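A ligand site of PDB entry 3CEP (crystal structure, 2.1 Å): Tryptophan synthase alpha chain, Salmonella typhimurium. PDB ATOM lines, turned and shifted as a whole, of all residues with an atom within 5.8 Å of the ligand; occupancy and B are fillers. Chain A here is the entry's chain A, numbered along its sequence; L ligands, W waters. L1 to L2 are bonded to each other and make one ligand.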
ATOM      1  N   PHE A  22     -11.199 -20.482  -0.689  1.00  0.00           N
ATOM      2  CA  PHE A  22     -12.436 -19.699  -0.876  1.00  0.00           C
ATOM      3  C   PHE A  22     -12.657 -19.327  -2.343  1.00  0.00           C
ATOM      4  O   PHE A  22     -11.715 -18.986  -3.052  1.00  0.00           O
ATOM      5  CB  PHE A  22     -12.434 -18.428  -0.015  1.00  0.00           C
ATOM      6  CG  PHE A  22     -13.456 -17.397  -0.456  1.00  0.00           C
ATOM      7  CD1 PHE A  22     -13.110 -16.416  -1.397  1.00  0.00           C
ATOM      8  CD2 PHE A  22     -14.738 -17.416   0.046  1.00  0.00           C
ATOM      9  CE1 PHE A  22     -14.049 -15.471  -1.820  1.00  0.00           C
ATOM     10  CE2 PHE A  22     -15.688 -16.471  -0.369  1.00  0.00           C
ATOM     11  CZ  PHE A  22     -15.338 -15.498  -1.306  1.00  0.00           C
ATOM     12  N   GLU A  49     -14.959 -22.587   1.744  1.00  0.00           N
ATOM     13  CA  GLU A  49     -15.583 -21.321   2.076  1.00  0.00           C
ATOM     14  C   GLU A  49     -16.101 -20.703   0.778  1.00  0.00           C
ATOM     15  O   GLU A  49     -15.349 -20.525  -0.173  1.00  0.00           O
ATOM     16  CB  GLU A  49     -14.619 -20.375   2.813  1.00  0.00           C
ATOM     17  CG  GLU A  49     -15.304 -19.141   3.384  1.00  0.00           C
ATOM     18  CD  GLU A  49     -14.315 -18.022   3.710  1.00  0.00           C
ATOM     19  OE1 GLU A  49     -14.705 -16.836   3.556  1.00  0.00           O
ATOM     20  OE2 GLU A  49     -13.168 -18.319   4.096  1.00  0.00           O
ATOM     21  N   ALA A  59     -15.102  -5.755   3.560  1.00  0.00           N
ATOM     22  CA  ALA A  59     -13.909  -6.425   4.098  1.00  0.00           C
ATOM     23  C   ALA A  59     -13.018  -7.009   2.997  1.00  0.00           C
ATOM     24  O   ALA A  59     -12.101  -7.773   3.270  1.00  0.00           O
ATOM     25  CB  ALA A  59     -14.306  -7.495   5.127  1.00  0.00           C
ATOM     26  N   ASP A  60     -13.263  -6.602   1.751  1.00  0.00           N
ATOM     27  CA  ASP A  60     -12.605  -7.203   0.606  1.00  0.00           C
ATOM     28  C   ASP A  60     -11.793  -6.213  -0.225  1.00  0.00           C
ATOM     29  O   ASP A  60     -12.248  -5.110  -0.515  1.00  0.00           O
ATOM     30  CB  ASP A  60     -13.626  -7.915  -0.286  1.00  0.00           C
ATOM     31  CG  ASP A  60     -14.048  -9.247   0.291  1.00  0.00           C
ATOM     32  OD1 ASP A  60     -13.181 -10.129   0.413  1.00  0.00           O
ATOM     33  OD2 ASP A  60     -15.254  -9.412   0.614  1.00  0.00           O
ATOM     34  N   ILE A  64     -11.188  -9.909  -4.705  1.00  0.00           N
ATOM     35  CA  ILE A  64     -12.507 -10.472  -4.409  1.00  0.00           C
ATOM     36  C   ILE A  64     -13.635  -9.504  -4.784  1.00  0.00           C
ATOM     37  O   ILE A  64     -14.728  -9.943  -5.162  1.00  0.00           O
ATOM     38  CB  ILE A  64     -12.610 -10.979  -2.950  1.00  0.00           C
ATOM     39  CG1 ILE A  64     -11.667 -12.172  -2.749  1.00  0.00           C
ATOM     40  CG2 ILE A  64     -14.027 -11.401  -2.642  1.00  0.00           C
ATOM     41  CD1 ILE A  64     -11.506 -12.629  -1.306  1.00  0.00           C
ATOM     42  N   LEU A 100     -19.433 -17.233   3.392  1.00  0.00           N
ATOM     43  CA  LEU A 100     -19.022 -15.898   3.782  1.00  0.00           C
ATOM     44  C   LEU A 100     -20.116 -14.949   3.335  1.00  0.00           C
ATOM     45  O   LEU A 100     -20.389 -14.820   2.134  1.00  0.00           O
ATOM     46  CB  LEU A 100     -17.670 -15.499   3.185  1.00  0.00           C
ATOM     47  CG  LEU A 100     -17.056 -14.152   3.637  1.00  0.00           C
ATOM     48  CD1 LEU A 100     -17.656 -12.913   2.915  1.00  0.00           C
ATOM     49  CD2 LEU A 100     -17.135 -14.003   5.147  1.00  0.00           C
ATOM     50  N   TYR A 102     -22.243 -11.044   4.017  1.00  0.00           N
ATOM     51  CA  TYR A 102     -22.370  -9.709   4.606  1.00  0.00           C
ATOM     52  C   TYR A 102     -23.755  -9.611   5.248  1.00  0.00           C
ATOM     53  O   TYR A 102     -24.696 -10.251   4.783  1.00  0.00           O
ATOM     54  CB  TYR A 102     -22.110  -8.605   3.577  1.00  0.00           C
ATOM     55  CG  TYR A 102     -20.625  -8.475   3.318  1.00  0.00           C
ATOM     56  CD1 TYR A 102     -19.825  -7.658   4.111  1.00  0.00           C
ATOM     57  CD2 TYR A 102     -20.001  -9.229   2.311  1.00  0.00           C
ATOM     58  CE1 TYR A 102     -18.459  -7.564   3.916  1.00  0.00           C
ATOM     59  CE2 TYR A 102     -18.622  -9.137   2.098  1.00  0.00           C
ATOM     60  CZ  TYR A 102     -17.864  -8.300   2.896  1.00  0.00           C
ATOM     61  OH  TYR A 102     -16.501  -8.200   2.687  1.00  0.00           O
ATOM     62  N   LEU A 127     -20.116 -17.272   8.171  1.00  0.00           N
ATOM     63  CA  LEU A 127     -19.319 -16.158   8.665  1.00  0.00           C
ATOM     64  C   LEU A 127     -19.963 -14.868   8.165  1.00  0.00           C
ATOM     65  O   LEU A 127     -20.062 -14.662   6.962  1.00  0.00           O
ATOM     66  CB  LEU A 127     -17.888 -16.247   8.149  1.00  0.00           C
ATOM     67  CG  LEU A 127     -16.689 -15.692   8.922  1.00  0.00           C
ATOM     68  CD1 LEU A 127     -15.512 -15.479   7.974  1.00  0.00           C
ATOM     69  CD2 LEU A 127     -16.976 -14.410   9.726  1.00  0.00           C
ATOM     70  N   ALA A 129     -19.195 -11.193   7.875  1.00  0.00           N
ATOM     71  CA  ALA A 129     -17.992 -10.343   7.936  1.00  0.00           C
ATOM     72  C   ALA A 129     -18.156  -9.043   8.738  1.00  0.00           C
ATOM     73  O   ALA A 129     -17.226  -8.614   9.423  1.00  0.00           O
ATOM     74  CB  ALA A 129     -17.509 -10.042   6.518  1.00  0.00           C
ATOM     75  N   ILE A 153     -14.582 -14.055  13.872  1.00  0.00           N
ATOM     76  CA  ILE A 153     -13.195 -13.695  13.635  1.00  0.00           C
ATOM     77  C   ILE A 153     -12.499 -13.317  14.932  1.00  0.00           C
ATOM     78  O   ILE A 153     -13.018 -12.532  15.732  1.00  0.00           O
ATOM     79  CB  ILE A 153     -13.078 -12.544  12.612  1.00  0.00           C
ATOM     80  CG1 ILE A 153     -13.500 -13.027  11.218  1.00  0.00           C
ATOM     81  CG2 ILE A 153     -11.656 -11.992  12.572  1.00  0.00           C
ATOM     82  CD1 ILE A 153     -13.721 -11.911  10.210  1.00  0.00           C
ATOM     83  N   TYR A 175     -12.229 -18.280  13.209  1.00  0.00           N
ATOM     84  CA  TYR A 175     -11.525 -17.584  12.137  1.00  0.00           C
ATOM     85  C   TYR A 175     -10.423 -16.734  12.744  1.00  0.00           C
ATOM     86  O   TYR A 175     -10.682 -15.712  13.401  1.00  0.00           O
ATOM     87  CB  TYR A 175     -12.468 -16.710  11.293  1.00  0.00           C
ATOM     88  CG  TYR A 175     -11.878 -16.289   9.952  1.00  0.00           C
ATOM     89  CD1 TYR A 175     -10.803 -15.413   9.887  1.00  0.00           C
ATOM     90  CD2 TYR A 175     -12.416 -16.778   8.753  1.00  0.00           C
ATOM     91  CE1 TYR A 175     -10.256 -15.029   8.660  1.00  0.00           C
ATOM     92  CE2 TYR A 175     -11.882 -16.389   7.521  1.00  0.00           C
ATOM     93  CZ  TYR A 175     -10.804 -15.523   7.483  1.00  0.00           C
ATOM     94  OH  TYR A 175     -10.277 -15.143   6.263  1.00  0.00           O
ATOM     95  N   ARG A 179      -3.992 -10.583  10.002  1.00  0.00           N
ATOM     96  CA  ARG A 179      -3.592  -9.159   9.963  1.00  0.00           C
ATOM     97  C   ARG A 179      -4.816  -8.271   9.860  1.00  0.00           C
ATOM     98  O   ARG A 179      -5.899  -8.730   9.481  1.00  0.00           O
ATOM     99  CB  ARG A 179      -2.678  -8.876   8.757  1.00  0.00           C
ATOM    100  CG  ARG A 179      -3.255  -9.314   7.399  1.00  0.00           C
ATOM    101  CD  ARG A 179      -2.773  -8.441   6.255  1.00  0.00           C
ATOM    102  NE  ARG A 179      -3.250  -8.935   4.963  1.00  0.00           N
ATOM    103  CZ  ARG A 179      -4.410  -8.619   4.403  1.00  0.00           C
ATOM    104  NH1 ARG A 179      -5.247  -7.774   5.001  1.00  0.00           N
ATOM    105  NH2 ARG A 179      -4.747  -9.139   3.227  1.00  0.00           N
ATOM    106  N   VAL A 182      -8.011  -5.497   4.688  1.00  0.00           N
ATOM    107  CA  VAL A 182      -9.025  -6.213   3.930  1.00  0.00           C
ATOM    108  C   VAL A 182      -8.373  -7.384   3.196  1.00  0.00           C
ATOM    109  O   VAL A 182      -7.153  -7.490   3.165  1.00  0.00           O
ATOM    110  CB  VAL A 182      -9.776  -5.285   2.921  1.00  0.00           C
ATOM    111  CG1 VAL A 182     -10.479  -4.148   3.656  1.00  0.00           C
ATOM    112  CG2 VAL A 182      -8.831  -4.729   1.858  1.00  0.00           C
ATOM    113  N   THR A 183      -9.189  -8.260   2.619  1.00  0.00           N
ATOM    114  CA  THR A 183      -8.661  -9.452   1.932  1.00  0.00           C
ATOM    115  C   THR A 183      -7.684  -9.056   0.827  1.00  0.00           C
ATOM    116  O   THR A 183      -7.836  -8.004   0.197  1.00  0.00           O
ATOM    117  CB  THR A 183      -9.794 -10.332   1.341  1.00  0.00           C
ATOM    118  OG1 THR A 183     -10.499  -9.600   0.329  1.00  0.00           O
ATOM    119  CG2 THR A 183     -10.758 -10.780   2.425  1.00  0.00           C
ATOM    120  N   GLY A 184      -6.670  -9.890   0.613  1.00  0.00           N
ATOM    121  CA  GLY A 184      -5.662  -9.615  -0.396  1.00  0.00           C
ATOM    122  C   GLY A 184      -4.474 -10.544  -0.296  1.00  0.00           C
ATOM    123  O   GLY A 184      -3.845 -10.642   0.764  1.00  0.00           O
ATOM    124  N   ALA A 185      -4.173 -11.210  -1.396  1.00  0.00           N
ATOM    125  CA  ALA A 185      -3.066 -12.161  -1.491  1.00  0.00           C
ATOM    126  C   ALA A 185      -1.681 -11.497  -1.364  1.00  0.00           C
ATOM    127  O   ALA A 185      -0.733 -12.110  -0.879  1.00  0.00           O
ATOM    128  CB  ALA A 185      -3.151 -12.951  -2.793  1.00  0.00           C
ATOM    129  N   GLY A 211      -6.637 -16.985   8.198  1.00  0.00           N
ATOM    130  CA  GLY A 211      -7.052 -16.423   6.911  1.00  0.00           C
ATOM    131  C   GLY A 211      -6.689 -14.957   6.771  1.00  0.00           C
ATOM    132  O   GLY A 211      -6.608 -14.226   7.778  1.00  0.00           O
ATOM    133  N   PHE A 212      -6.506 -14.547   5.509  1.00  0.00           N
ATOM    134  CA  PHE A 212      -6.040 -13.202   5.067  1.00  0.00           C
ATOM    135  C   PHE A 212      -4.579 -13.224   4.664  1.00  0.00           C
ATOM    136  O   PHE A 212      -3.687 -13.370   5.504  1.00  0.00           O
ATOM    137  CB  PHE A 212      -6.290 -12.093   6.098  1.00  0.00           C
ATOM    138  CG  PHE A 212      -7.651 -11.459   6.017  1.00  0.00           C
ATOM    139  CD1 PHE A 212      -8.811 -12.242   6.028  1.00  0.00           C
ATOM    140  CD2 PHE A 212      -7.782 -10.079   5.977  1.00  0.00           C
ATOM    141  CE1 PHE A 212     -10.053 -11.652   5.968  1.00  0.00           C
ATOM    142  CE2 PHE A 212      -9.024  -9.489   5.918  1.00  0.00           C
ATOM    143  CZ  PHE A 212     -10.163 -10.268   5.920  1.00  0.00           C
ATOM    144  N   GLY A 213      -4.321 -13.088   3.358  1.00  0.00           N
ATOM    145  CA  GLY A 213      -2.967 -13.010   2.839  1.00  0.00           C
ATOM    146  C   GLY A 213      -2.198 -14.323   2.699  1.00  0.00           C
ATOM    147  O   GLY A 213      -1.004 -14.304   2.429  1.00  0.00           O
ATOM    148  N   ILE A 214      -2.883 -15.453   2.869  1.00  0.00           N
ATOM    149  CA  ILE A 214      -2.258 -16.762   2.695  1.00  0.00           C
ATOM    150  C   ILE A 214      -2.295 -17.139   1.214  1.00  0.00           C
ATOM    151  O   ILE A 214      -3.368 -17.391   0.660  1.00  0.00           O
ATOM    152  CB  ILE A 214      -2.969 -17.873   3.529  1.00  0.00           C
ATOM    153  CG1 ILE A 214      -3.228 -17.425   4.984  1.00  0.00           C
ATOM    154  CG2 ILE A 214      -2.197 -19.199   3.460  1.00  0.00           C
ATOM    155  CD1 ILE A 214      -1.993 -17.119   5.804  1.00  0.00           C
ATOM    156  N   ILE A 232      -6.668 -20.797   5.392  1.00  0.00           N
ATOM    157  CA  ILE A 232      -7.654 -20.434   4.394  1.00  0.00           C
ATOM    158  C   ILE A 232      -7.004 -19.528   3.362  1.00  0.00           C
ATOM    159  O   ILE A 232      -6.318 -18.566   3.714  1.00  0.00           O
ATOM    160  CB  ILE A 232      -8.870 -19.679   5.030  1.00  0.00           C
ATOM    161  CG1 ILE A 232      -9.501 -20.493   6.162  1.00  0.00           C
ATOM    162  CG2 ILE A 232      -9.928 -19.345   3.962  1.00  0.00           C
ATOM    163  CD1 ILE A 232     -10.324 -19.662   7.119  1.00  0.00           C
ATOM    164  N   SER A 233      -7.197 -19.851   2.088  1.00  0.00           N
ATOM    165  CA  SER A 233      -6.728 -19.002   1.006  1.00  0.00           C
ATOM    166  C   SER A 233      -7.909 -18.588   0.120  1.00  0.00           C
ATOM    167  O   SER A 233      -8.634 -19.451  -0.388  1.00  0.00           O
ATOM    168  CB  SER A 233      -5.670 -19.731   0.171  1.00  0.00           C
ATOM    169  OG  SER A 233      -5.191 -18.909  -0.877  1.00  0.00           O
ATOM    170  N   GLY A 234      -8.088 -17.284  -0.033  1.00  0.00           N
ATOM    171  CA  GLY A 234      -9.169 -16.734  -0.850  1.00  0.00           C
ATOM    172  C   GLY A 234      -8.668 -16.033  -2.098  1.00  0.00           C
ATOM    173  O   GLY A 234      -8.778 -16.574  -3.205  1.00  0.00           O
ATOM    174  N   SER A 235      -8.103 -14.841  -1.926  1.00  0.00           N
ATOM    175  CA  SER A 235      -7.660 -14.007  -3.041  1.00  0.00           C
ATOM    176  C   SER A 235      -6.690 -14.725  -3.997  1.00  0.00           C
ATOM    177  O   SER A 235      -6.772 -14.530  -5.214  1.00  0.00           O
ATOM    178  CB  SER A 235      -7.045 -12.692  -2.532  1.00  0.00           C
ATOM    179  OG  SER A 235      -7.987 -11.943  -1.789  1.00  0.00           O
ATOM    180  N   ALA A 236      -5.813 -15.549  -3.437  1.00  0.00           N
ATOM    181  CA  ALA A 236      -4.873 -16.359  -4.233  1.00  0.00           C
ATOM    182  C   ALA A 236      -5.611 -17.271  -5.206  1.00  0.00           C
ATOM    183  O   ALA A 236      -5.247 -17.355  -6.372  1.00  0.00           O
ATOM    184  CB  ALA A 236      -3.972 -17.172  -3.323  1.00  0.00           C
HETATM  185  O1  LIG L   1     -11.588 -16.326   3.827  1.00  0.00           O
HETATM  186  C1  LIG L   1     -11.699 -15.092   3.366  1.00  0.00           C
HETATM  187  C2  LIG L   1     -10.612 -14.734   2.431  1.00  0.00           C
HETATM  188  O2  LIG L   1     -10.983 -14.050   1.358  1.00  0.00           O
HETATM  189  C3  LIG L   1      -9.575 -13.962   3.085  1.00  0.00           C
HETATM  190  O3  LIG L   1      -8.264 -14.471   2.725  1.00  0.00           O
HETATM  191  O4  LIG L   1      -6.913 -12.555   1.933  1.00  0.00           O
HETATM  192  O5  LIG L   1      -8.631 -13.559   0.376  1.00  0.00           O
HETATM  193  O6  LIG L   1      -6.603 -14.899   1.035  1.00  0.00           O
HETATM  194  P1  LIG L   1      -7.569 -13.805   1.423  1.00  0.00           P
HETATM  195  N1  LG2 L   2     -13.143 -14.786   3.098  1.00  0.00           N
HETATM  196  C1  LG2 L   2     -13.505 -14.353   1.718  1.00  0.00           C
HETATM  197  C2  LG2 L   2     -13.975 -12.869   1.761  1.00  0.00           C
HETATM  198  C3  LG2 L   2     -13.890 -12.593   3.236  1.00  0.00           C
HETATM  199  C4  LG2 L   2     -14.218 -11.424   3.888  1.00  0.00           C
HETATM  200  C5  LG2 L   2     -14.072 -11.393   5.295  1.00  0.00           C
HETATM  201  C6  LG2 L   2     -13.602 -12.518   6.001  1.00  0.00           C
HETATM  202  C7  LG2 L   2     -13.277 -13.702   5.320  1.00  0.00           C
HETATM  203  C8  LG2 L   2     -13.431 -13.718   3.928  1.00  0.00           C
HETATM  204  O   HOH W   1      -4.748 -15.308  -0.772  1.00  0.00           O
HETATM  205  O   HOH W   2      -6.002 -16.035   3.422  1.00  0.00           O
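N of Gly 184 sits at hydrogen-bond distance from O4 of LIG L1 (3.0 Å).
O1 of LIG L1 is in hydrogen-bond range of OE2 of Glu 49, at 2.6 Å.
OG of Ser 235 is in hydrogen-bond range of O5 of LIG L1 (2.8 Å).
O5 of LIG L1 lies within hydrogen-bond range of N of Ser 235 (2.7 Å).
The backbone NH (N) of Gly 234 sits at hydrogen-bond distance from an oxygen (O6) of LIG L1, at 3.0 Å.
N of Phe 212 is in hydrogen-bond range of O3 of LIG L1 (3.3 Å).
An oxygen (O4) of LIG L1 sits at hydrogen-bond distance from the backbone NH (N) of Gly 213 (3.0 Å).
The side-chain hydroxyl (OH) of Tyr 175 lies within hydrogen-bond range of an oxygen (O1) of LIG L1.
The side-chain carboxylate (OD2) of Asp 60 is in hydrogen-bond range of the side-chain hydroxyl (OH) of Tyr 102, at 2.7 Å.
The side-chain carboxylate (OD1) of Asp 60 sits at hydrogen-bond distance from the side-chain hydroxyl (OG1) of Thr 183.
O of Ala 59 is in hydrogen-bond range of N of Thr 183, 3.0 Å away.
The backbone NH (N) of Ala 59 is in hydrogen-bond range of the side-chain hydroxyl (OH) of Tyr 102, at 2.9 Å.
The backbone NH (N) of Gly 184 sits at hydrogen-bond distance from the side-chain hydroxyl (OG) of Ser 235 (3.4 Å).
The backbone carbonyl oxygen of Gly 184 lies within hydrogen-bond range of the guanidinium group of Arg 179 (3.0 Å).
The backbone NH (N) of Phe 22 sits at hydrogen-bond distance from the backbone carbonyl oxygen (O) of Ser 233, at 2.8 Å.
CE2 of Phe 22 touches C1 of LG2 L2, at 3.7 Å.
Ala 59 touches the ligand.
Asp 60 touches the ligand.
CD1 of Ile 64 touches O2 of LIG L1, 3.1 Å away.
CG of Leu 100 touches C3 of LG2 L2 (3.6 Å).
CD1 of Leu 127 touches C7 of LG2 L2 (3.9 Å).
CB of Ala 129 touches C5 of LG2 L2, 3.9 Å away.
Thr 183 touches the ligand.
CG2 of Ile 232 touches O1 of LIG L1, 3.4 Å away.
Hydrophobic or aromatic side chains that line the ligand: Phe 22, Ala 59, Ile 64, Leu 100, Leu 127, Ala 129, Tyr 175, Phe 212 and Ile 232.
16 residues have an atom within 4 Å of the ligand: Phe 22, Glu 49, Ala 59, Asp 60, Ile 64, Leu 100, Leu 127, Ala 129, Tyr 175, Thr 183, Gly 184, Phe 212, Gly 213, Ile 232, Gly 234 and Ser 235.
Water W1 lies within hydrogen-bond range of an oxygen (O6) of LIG L1 (2.6 Å), the backbone carbonyl oxygen (O) of Ile 214 (2.9 Å) and the backbone NH (N) of Ala 236 (2.9 Å).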
